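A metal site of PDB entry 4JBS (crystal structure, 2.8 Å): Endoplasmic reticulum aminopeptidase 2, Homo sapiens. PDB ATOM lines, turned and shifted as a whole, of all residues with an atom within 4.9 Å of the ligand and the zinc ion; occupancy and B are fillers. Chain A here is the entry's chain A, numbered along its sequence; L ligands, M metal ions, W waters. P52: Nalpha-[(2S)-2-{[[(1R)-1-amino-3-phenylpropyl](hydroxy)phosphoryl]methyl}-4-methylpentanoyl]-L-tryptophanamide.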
ATOM      1  N   GLU A 200      38.998   3.968  -2.916  1.00  0.00           N
ATOM      2  CA  GLU A 200      38.660   3.301  -1.653  1.00  0.00           C
ATOM      3  C   GLU A 200      38.594   1.787  -1.798  1.00  0.00           C
ATOM      4  O   GLU A 200      38.003   1.282  -2.756  1.00  0.00           O
ATOM      5  CB  GLU A 200      37.357   3.840  -1.070  1.00  0.00           C
ATOM      6  CG  GLU A 200      37.175   3.486   0.395  1.00  0.00           C
ATOM      7  CD  GLU A 200      35.825   3.893   0.930  1.00  0.00           C
ATOM      8  OE1 GLU A 200      34.972   4.293   0.114  1.00  0.00           O
ATOM      9  OE2 GLU A 200      35.613   3.794   2.152  1.00  0.00           O
ATOM     10  N   PRO A 201      39.197   1.051  -0.846  1.00  0.00           N
ATOM     11  CA  PRO A 201      39.946   1.647   0.258  1.00  0.00           C
ATOM     12  C   PRO A 201      41.442   1.733  -0.021  1.00  0.00           C
ATOM     13  O   PRO A 201      42.124   2.625   0.490  1.00  0.00           O
ATOM     14  CB  PRO A 201      39.711   0.646   1.411  1.00  0.00           C
ATOM     15  CG  PRO A 201      38.933  -0.514   0.822  1.00  0.00           C
ATOM     16  CD  PRO A 201      39.035  -0.394  -0.666  1.00  0.00           C
ATOM     17  N   PRO A 333      31.394   0.738  -7.919  1.00  0.00           N
ATOM     18  CA  PRO A 333      30.631   1.066  -6.719  1.00  0.00           C
ATOM     19  C   PRO A 333      29.302   1.713  -7.084  1.00  0.00           C
ATOM     20  O   PRO A 333      29.084   2.024  -8.255  1.00  0.00           O
ATOM     21  CB  PRO A 333      31.520   2.087  -5.998  1.00  0.00           C
ATOM     22  CG  PRO A 333      32.830   2.085  -6.717  1.00  0.00           C
ATOM     23  CD  PRO A 333      32.557   1.617  -8.099  1.00  0.00           C
ATOM     24  N   GLY A 334      28.414   1.906  -6.104  1.00  0.00           N
ATOM     25  CA  GLY A 334      27.189   2.638  -6.342  1.00  0.00           C
ATOM     26  C   GLY A 334      27.513   4.096  -6.586  1.00  0.00           C
ATOM     27  O   GLY A 334      26.943   4.738  -7.472  1.00  0.00           O
ATOM     28  N   ALA A 335      28.448   4.608  -5.794  1.00  0.00           N
ATOM     29  CA  ALA A 335      29.017   5.949  -5.981  1.00  0.00           C
ATOM     30  C   ALA A 335      30.220   6.120  -5.036  1.00  0.00           C
ATOM     31  O   ALA A 335      30.432   5.289  -4.156  1.00  0.00           O
ATOM     32  CB  ALA A 335      27.962   7.007  -5.714  1.00  0.00           C
ATOM     33  N   MET A 336      30.998   7.179  -5.210  1.00  0.00           N
ATOM     34  CA  MET A 336      32.137   7.444  -4.320  1.00  0.00           C
ATOM     35  C   MET A 336      32.240   8.906  -3.904  1.00  0.00           C
ATOM     36  O   MET A 336      32.134   9.820  -4.727  1.00  0.00           O
ATOM     37  CB  MET A 336      33.451   6.969  -4.944  1.00  0.00           C
ATOM     38  CG  MET A 336      34.668   7.181  -4.046  1.00  0.00           C
ATOM     39  SD  MET A 336      34.549   6.310  -2.460  1.00  0.00           S
ATOM     40  CE  MET A 336      35.862   7.101  -1.523  1.00  0.00           C
ATOM     41  N   GLU A 337      32.462   9.120  -2.624  1.00  0.00           N
ATOM     42  CA  GLU A 337      32.318  10.442  -2.032  1.00  0.00           C
ATOM     43  C   GLU A 337      33.561  11.320  -2.131  1.00  0.00           C
ATOM     44  O   GLU A 337      33.730  12.243  -1.327  1.00  0.00           O
ATOM     45  CB  GLU A 337      31.870  10.315  -0.570  1.00  0.00           C
ATOM     46  CG  GLU A 337      32.951   9.863   0.413  1.00  0.00           C
ATOM     47  CD  GLU A 337      32.970   8.365   0.661  1.00  0.00           C
ATOM     48  OE1 GLU A 337      33.566   7.938   1.685  1.00  0.00           O
ATOM     49  OE2 GLU A 337      32.400   7.602  -0.155  1.00  0.00           O
ATOM     50  N   TRP A 363      15.493   6.504  -5.164  1.00  0.00           N
ATOM     51  CA  TRP A 363      16.848   5.965  -5.192  1.00  0.00           C
ATOM     52  C   TRP A 363      17.881   7.079  -5.336  1.00  0.00           C
ATOM     53  O   TRP A 363      18.674   7.307  -4.407  1.00  0.00           O
ATOM     54  CB  TRP A 363      17.013   4.959  -6.340  1.00  0.00           C
ATOM     55  CG  TRP A 363      18.422   4.374  -6.492  1.00  0.00           C
ATOM     56  CD1 TRP A 363      19.245   4.480  -7.579  1.00  0.00           C
ATOM     57  CD2 TRP A 363      19.133   3.587  -5.523  1.00  0.00           C
ATOM     58  NE1 TRP A 363      20.427   3.813  -7.341  1.00  0.00           N
ATOM     59  CE2 TRP A 363      20.385   3.267  -6.090  1.00  0.00           C
ATOM     60  CE3 TRP A 363      18.838   3.143  -4.235  1.00  0.00           C
ATOM     61  CZ2 TRP A 363      21.333   2.501  -5.400  1.00  0.00           C
ATOM     62  CZ3 TRP A 363      19.789   2.385  -3.556  1.00  0.00           C
ATOM     63  CH2 TRP A 363      21.022   2.068  -4.144  1.00  0.00           C
ATOM     64  N   VAL A 367      20.827   8.108  -2.689  1.00  0.00           N
ATOM     65  CA  VAL A 367      22.274   8.000  -2.887  1.00  0.00           C
ATOM     66  C   VAL A 367      22.977   9.355  -2.935  1.00  0.00           C
ATOM     67  O   VAL A 367      24.118   9.494  -2.501  1.00  0.00           O
ATOM     68  CB  VAL A 367      22.666   7.086  -4.092  1.00  0.00           C
ATOM     69  CG1 VAL A 367      21.524   6.946  -5.062  1.00  0.00           C
ATOM     70  CG2 VAL A 367      23.925   7.590  -4.780  1.00  0.00           C
ATOM     71  N   HIS A 370      23.229  10.321   0.646  1.00  0.00           N
ATOM     72  CA  HIS A 370      24.309   9.526   1.208  1.00  0.00           C
ATOM     73  C   HIS A 370      25.678  10.141   0.957  1.00  0.00           C
ATOM     74  O   HIS A 370      26.483  10.301   1.877  1.00  0.00           O
ATOM     75  CB  HIS A 370      24.276   8.103   0.644  1.00  0.00           C
ATOM     76  CG  HIS A 370      25.211   7.150   1.324  1.00  0.00           C
ATOM     77  ND1 HIS A 370      24.880   6.496   2.483  1.00  0.00           N
ATOM     78  CD2 HIS A 370      26.454   6.722   0.986  1.00  0.00           C
ATOM     79  CE1 HIS A 370      25.884   5.702   2.843  1.00  0.00           C
ATOM     80  NE2 HIS A 370      26.840   5.820   1.946  1.00  0.00           N
ATOM     81  N   GLU A 371      25.957  10.500  -0.297  1.00  0.00           N
ATOM     82  CA  GLU A 371      27.292  10.979  -0.667  1.00  0.00           C
ATOM     83  C   GLU A 371      27.601  12.353  -0.088  1.00  0.00           C
ATOM     84  O   GLU A 371      28.740  12.620   0.286  1.00  0.00           O
ATOM     85  CB  GLU A 371      27.477  10.987  -2.179  1.00  0.00           C
ATOM     86  CG  GLU A 371      27.260   9.636  -2.834  1.00  0.00           C
ATOM     87  CD  GLU A 371      28.212   8.575  -2.329  1.00  0.00           C
ATOM     88  OE1 GLU A 371      27.769   7.412  -2.182  1.00  0.00           O
ATOM     89  OE2 GLU A 371      29.389   8.886  -2.075  1.00  0.00           O
ATOM     90  N   HIS A 374      28.672  12.297   3.405  1.00  0.00           N
ATOM     91  CA  HIS A 374      30.043  11.796   3.514  1.00  0.00           C
ATOM     92  C   HIS A 374      31.060  12.920   3.600  1.00  0.00           C
ATOM     93  O   HIS A 374      32.070  12.793   4.301  1.00  0.00           O
ATOM     94  CB  HIS A 374      30.390  10.907   2.315  1.00  0.00           C
ATOM     95  CG  HIS A 374      30.148   9.447   2.569  1.00  0.00           C
ATOM     96  ND1 HIS A 374      30.316   8.866   3.803  1.00  0.00           N
ATOM     97  CD2 HIS A 374      29.763   8.455   1.727  1.00  0.00           C
ATOM     98  CE1 HIS A 374      30.033   7.574   3.717  1.00  0.00           C
ATOM     99  NE2 HIS A 374      29.708   7.302   2.467  1.00  0.00           N
ATOM    100  N   LYS A 392      31.806   6.107   9.341  1.00  0.00           N
ATOM    101  CA  LYS A 392      31.612   6.807   8.077  1.00  0.00           C
ATOM    102  C   LYS A 392      30.315   6.325   7.446  1.00  0.00           C
ATOM    103  O   LYS A 392      29.425   7.123   7.134  1.00  0.00           O
ATOM    104  CB  LYS A 392      32.804   6.523   7.160  1.00  0.00           C
ATOM    105  CG  LYS A 392      32.790   7.218   5.805  1.00  0.00           C
ATOM    106  CD  LYS A 392      34.151   7.108   5.102  1.00  0.00           C
ATOM    107  CE  LYS A 392      34.359   5.745   4.446  1.00  0.00           C
ATOM    108  NZ  LYS A 392      33.707   5.663   3.107  1.00  0.00           N
ATOM    109  N   GLU A 393      30.196   5.015   7.290  1.00  0.00           N
ATOM    110  CA  GLU A 393      29.091   4.394   6.557  1.00  0.00           C
ATOM    111  C   GLU A 393      27.752   4.332   7.277  1.00  0.00           C
ATOM    112  O   GLU A 393      26.710   4.612   6.674  1.00  0.00           O
ATOM    113  CB  GLU A 393      29.512   2.998   6.086  1.00  0.00           C
ATOM    114  CG  GLU A 393      30.691   3.018   5.131  1.00  0.00           C
ATOM    115  CD  GLU A 393      30.432   3.891   3.902  1.00  0.00           C
ATOM    116  OE1 GLU A 393      29.275   4.293   3.706  1.00  0.00           O
ATOM    117  OE2 GLU A 393      31.385   4.159   3.142  1.00  0.00           O
ATOM    118  N   ALA A 396      26.393   8.049   7.348  1.00  0.00           N
ATOM    119  CA  ALA A 396      25.907   8.460   6.041  1.00  0.00           C
ATOM    120  C   ALA A 396      24.563   7.793   5.753  1.00  0.00           C
ATOM    121  O   ALA A 396      23.604   8.454   5.373  1.00  0.00           O
ATOM    122  CB  ALA A 396      26.913   8.090   4.967  1.00  0.00           C
ATOM    123  N   GLU A 400      20.820   9.773   5.410  1.00  0.00           N
ATOM    124  CA  GLU A 400      19.905   9.601   4.271  1.00  0.00           C
ATOM    125  C   GLU A 400      18.495   9.872   4.766  1.00  0.00           C
ATOM    126  O   GLU A 400      17.760  10.666   4.191  1.00  0.00           O
ATOM    127  CB  GLU A 400      19.962   8.165   3.728  1.00  0.00           C
ATOM    128  CG  GLU A 400      21.209   7.798   2.926  1.00  0.00           C
ATOM    129  CD  GLU A 400      21.126   6.380   2.361  1.00  0.00           C
ATOM    130  OE1 GLU A 400      19.998   5.862   2.220  1.00  0.00           O
ATOM    131  OE2 GLU A 400      22.179   5.772   2.064  1.00  0.00           O
ATOM    132  N   PHE A 450      32.590  -3.712   4.288  1.00  0.00           N
ATOM    133  CA  PHE A 450      31.504  -2.941   3.699  1.00  0.00           C
ATOM    134  C   PHE A 450      30.301  -3.827   3.495  1.00  0.00           C
ATOM    135  O   PHE A 450      30.207  -4.558   2.518  1.00  0.00           O
ATOM    136  CB  PHE A 450      31.945  -2.327   2.363  1.00  0.00           C
ATOM    137  CG  PHE A 450      33.051  -1.317   2.497  1.00  0.00           C
ATOM    138  CD1 PHE A 450      32.764  -0.014   2.840  1.00  0.00           C
ATOM    139  CD2 PHE A 450      34.360  -1.681   2.290  1.00  0.00           C
ATOM    140  CE1 PHE A 450      33.775   0.916   2.957  1.00  0.00           C
ATOM    141  CE2 PHE A 450      35.380  -0.752   2.418  1.00  0.00           C
ATOM    142  CZ  PHE A 450      35.081   0.543   2.752  1.00  0.00           C
ATOM    143  N   ASP A 451      29.373  -3.776   4.436  1.00  0.00           N
ATOM    144  CA  ASP A 451      28.203  -4.640   4.370  1.00  0.00           C
ATOM    145  C   ASP A 451      27.064  -4.078   5.202  1.00  0.00           C
ATOM    146  O   ASP A 451      27.157  -2.983   5.747  1.00  0.00           O
ATOM    147  CB  ASP A 451      28.563  -6.047   4.833  1.00  0.00           C
ATOM    148  CG  ASP A 451      28.885  -6.107   6.308  1.00  0.00           C
ATOM    149  OD1 ASP A 451      28.799  -5.074   6.986  1.00  0.00           O
ATOM    150  OD2 ASP A 451      29.230  -7.214   6.774  1.00  0.00           O
ATOM    151  N   GLU A 452      25.988  -4.848   5.303  1.00  0.00           N
ATOM    152  CA  GLU A 452      24.776  -4.378   5.958  1.00  0.00           C
ATOM    153  C   GLU A 452      24.922  -4.254   7.466  1.00  0.00           C
ATOM    154  O   GLU A 452      23.988  -3.831   8.146  1.00  0.00           O
ATOM    155  CB  GLU A 452      23.603  -5.259   5.581  1.00  0.00           C
ATOM    156  CG  GLU A 452      24.023  -6.539   4.909  1.00  0.00           C
ATOM    157  CD  GLU A 452      23.230  -6.808   3.662  1.00  0.00           C
ATOM    158  OE1 GLU A 452      21.982  -6.822   3.736  1.00  0.00           O
ATOM    159  OE2 GLU A 452      23.854  -6.988   2.592  1.00  0.00           O
ATOM    160  N   TYR A 455      26.772  -0.622   7.553  1.00  0.00           N
ATOM    161  CA  TYR A 455      25.839   0.311   6.948  1.00  0.00           C
ATOM    162  C   TYR A 455      24.481   0.326   7.655  1.00  0.00           C
ATOM    163  O   TYR A 455      24.157   1.268   8.369  1.00  0.00           O
ATOM    164  CB  TYR A 455      25.648   0.002   5.459  1.00  0.00           C
ATOM    165  CG  TYR A 455      26.783   0.444   4.549  1.00  0.00           C
ATOM    166  CD1 TYR A 455      28.040  -0.131   4.640  1.00  0.00           C
ATOM    167  CD2 TYR A 455      26.581   1.441   3.603  1.00  0.00           C
ATOM    168  CE1 TYR A 455      29.069   0.281   3.806  1.00  0.00           C
ATOM    169  CE2 TYR A 455      27.608   1.842   2.762  1.00  0.00           C
ATOM    170  CZ  TYR A 455      28.842   1.265   2.863  1.00  0.00           C
ATOM    171  OH  TYR A 455      29.860   1.670   2.031  1.00  0.00           O
ATOM    172  N   TYR A 892      32.370  -6.368  -3.896  1.00  0.00           N
ATOM    173  CA  TYR A 892      30.939  -6.570  -3.761  1.00  0.00           C
ATOM    174  C   TYR A 892      30.422  -7.443  -4.894  1.00  0.00           C
ATOM    175  O   TYR A 892      29.527  -8.261  -4.696  1.00  0.00           O
ATOM    176  CB  TYR A 892      30.179  -5.250  -3.741  1.00  0.00           C
ATOM    177  CG  TYR A 892      28.773  -5.387  -3.211  1.00  0.00           C
ATOM    178  CD1 TYR A 892      28.529  -5.507  -1.854  1.00  0.00           C
ATOM    179  CD2 TYR A 892      27.679  -5.388  -4.083  1.00  0.00           C
ATOM    180  CE1 TYR A 892      27.242  -5.633  -1.367  1.00  0.00           C
ATOM    181  CE2 TYR A 892      26.392  -5.514  -3.596  1.00  0.00           C
ATOM    182  CZ  TYR A 892      26.177  -5.643  -2.237  1.00  0.00           C
ATOM    183  OH  TYR A 892      24.893  -5.761  -1.762  1.00  0.00           O
ATOM    184  N   ARG A 895      31.337 -11.125  -4.005  1.00  0.00           N
ATOM    185  CA  ARG A 895      30.587 -11.502  -2.825  1.00  0.00           C
ATOM    186  C   ARG A 895      29.116 -11.687  -3.178  1.00  0.00           C
ATOM    187  O   ARG A 895      28.433 -12.558  -2.650  1.00  0.00           O
ATOM    188  CB  ARG A 895      30.720 -10.446  -1.728  1.00  0.00           C
ATOM    189  CG  ARG A 895      29.600 -10.505  -0.707  1.00  0.00           C
ATOM    190  CD  ARG A 895      29.991  -9.891   0.621  1.00  0.00           C
ATOM    191  NE  ARG A 895      29.666  -8.472   0.692  1.00  0.00           N
ATOM    192  CZ  ARG A 895      30.564  -7.497   0.814  1.00  0.00           C
ATOM    193  NH1 ARG A 895      31.859  -7.801   0.881  1.00  0.00           N
ATOM    194  NH2 ARG A 895      30.180  -6.243   0.861  1.00  0.00           N
HETATM  195  O1  P52 L   1      29.566   6.108  -0.290  1.00  0.00           O
HETATM  196  O2  P52 L   1      29.258   3.902   0.589  1.00  0.00           O
HETATM  197  C1  P52 L   1      32.486   2.653  -2.055  1.00  0.00           C
HETATM  198  C2  P52 L   1      33.142   1.300  -1.816  1.00  0.00           C
HETATM  199  C3  P52 L   1      34.490   1.092  -1.572  1.00  0.00           C
HETATM  200  C4  P52 L   1      34.932  -0.211  -1.359  1.00  0.00           C
HETATM  201  C5  P52 L   1      34.122  -1.301  -1.372  1.00  0.00           C
HETATM  202  C6  P52 L   1      32.748  -1.106  -1.614  1.00  0.00           C
HETATM  203  N1  P52 L   1      32.232   4.903   0.091  1.00  0.00           N
HETATM  204  C7  P52 L   1      32.287   0.201  -1.838  1.00  0.00           C
HETATM  205  C8  P52 L   1      31.653   2.996  -0.827  1.00  0.00           C
HETATM  206  C9  P52 L   1      31.472   4.335  -0.784  1.00  0.00           C
HETATM  207  C10 P52 L   1      28.378   1.774  -1.801  1.00  0.00           C
HETATM  208  C11 P52 L   1      28.968   4.299  -1.881  1.00  0.00           C
HETATM  209  C12 P52 L   1      27.883   3.199  -1.617  1.00  0.00           C
HETATM  210  N2  P52 L   1      28.065   1.054  -2.990  1.00  0.00           N
HETATM  211  C13 P52 L   1      26.672   3.463  -2.570  1.00  0.00           C
HETATM  212  C14 P52 L   1      25.301   3.500  -1.886  1.00  0.00           C
HETATM  213  C15 P52 L   1      24.684   4.904  -1.931  1.00  0.00           C
HETATM  214  C16 P52 L   1      25.493   3.031  -0.436  1.00  0.00           C
HETATM  215  C17 P52 L   1      27.316  -0.045  -3.599  1.00  0.00           C
HETATM  216  N3  P52 L   1      29.055  -1.678   0.269  1.00  0.00           N
HETATM  217  P1  P52 L   1      29.750   4.681  -0.541  1.00  0.00           P
HETATM  218  C18 P52 L   1      25.854  -0.061  -3.149  1.00  0.00           C
HETATM  219  C19 P52 L   1      27.973  -1.382  -3.261  1.00  0.00           C
HETATM  220  C20 P52 L   1      28.145  -1.599  -1.791  1.00  0.00           C
HETATM  221  C21 P52 L   1      29.275  -1.387  -1.054  1.00  0.00           C
HETATM  222  C22 P52 L   1      27.150  -2.058  -0.859  1.00  0.00           C
HETATM  223  C23 P52 L   1      27.747  -2.096   0.417  1.00  0.00           C
HETATM  224  C24 P52 L   1      25.809  -2.445  -0.979  1.00  0.00           C
HETATM  225  C25 P52 L   1      27.063  -2.498   1.560  1.00  0.00           C
HETATM  226  C26 P52 L   1      25.116  -2.845   0.164  1.00  0.00           C
HETATM  227  C27 P52 L   1      25.750  -2.866   1.417  1.00  0.00           C
HETATM  228  O4  P52 L   1      25.550   0.328  -2.023  1.00  0.00           O
HETATM  229  N4  P52 L   1      24.856  -0.653  -3.968  1.00  0.00           N
HETATM  230 ZN    ZN M   1      28.887   5.456   2.067  1.00  0.00          ZN
HETATM  231  O   HOH W   1      22.887  -0.865  -2.136  1.00  0.00           O
HETATM  232  O   HOH W   2      25.603  -0.586  -6.354  1.00  0.00           O
HETATM  233  O   HOH W   3      35.965   2.672  -4.234  1.00  0.00           O
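The side-chain carboxylate of Glu 393 is in salt-bridge range of the side-chain amino group of Lys 392, at 2.8 Å.
The side-chain carboxylate (OE1) of Glu 337 lies within salt-bridge range of the side-chain amino group (NZ) of Lys 392 (2.7 Å).
OE2 of Glu 400 is in hydrogen-bond range of ND1 of His 370, 2.8 Å away.
N of Glu 337 lies within hydrogen-bond range of OE2 of Glu 371 (3.1 Å).
The side-chain carboxylate of Glu 200 is in salt-bridge range of the side-chain amino group of Lys 392.
The side-chain hydroxyl of Tyr 455 lies close to the side-chain carboxylate of Glu 393 (3.1 Å).
Merely in contact with the zinc ion: Tyr 455 (3.9 Å).
Four residues have an atom within 4 Å of the zinc ion: His 370, His 374, Glu 393 and Tyr 455.
The nearest printed residue that does not touch the zinc ion is Ala 396 (4.4 Å).
The side-chain amino group (NZ) of Lys 392 sits close to a nitrogen (N1) of the ligand, 3.4 Å away.
The side-chain hydroxyl of Tyr 455 lies close to an oxygen (O2) of the ligand (2.7 Å).
A nitrogen (N1) of the ligand is in salt-bridge range of the side-chain carboxylate of Glu 337, 2.7 Å away.
A nitrogen (N1) of the ligand is in hydrogen-bond range of the side-chain sulfur (SD) of Met 336.
The backbone NH (N) of Gly 334 lies close to a nitrogen (N2) of the ligand (3.2 Å).
The side-chain carboxylate of Glu 200 lies within salt-bridge range of a nitrogen (N1) of the ligand (2.8 Å).
The side-chain carboxylate of Glu 371 lies close to an oxygen (O1) of the ligand (2.9 Å).
O of Ala 335 touches C11 of the ligand, 2.9 Å away.
Val 367 touches the ligand (CB to C15, 3.7 Å).
Phe 450 touches the ligand (CB to N3, 3.6 Å).
CA of Asp 451 touches C25 of the ligand, 3.7 Å away.
Tyr 892 touches the ligand (CZ to C24, 3.5 Å).
Within 4 Å of the ligand: Glu 200, Gly 334, Ala 335, Met 336, Glu 337, Val 367, His 370, Glu 371, His 374, Lys 392, Glu 393, Phe 450, Asp 451, Tyr 455 and Tyr 892.
The zinc ion is bound by the side-chain carboxylate (OE1) of Glu 393 (2.0 Å), a ring nitrogen (NE2) of His 374 (2.1 Å), a ring nitrogen (NE2) of His 370 (2.1 Å), an oxygen (O2) of the ligand (2.2 Å) and an oxygen (O1) of the ligand (2.5 Å).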
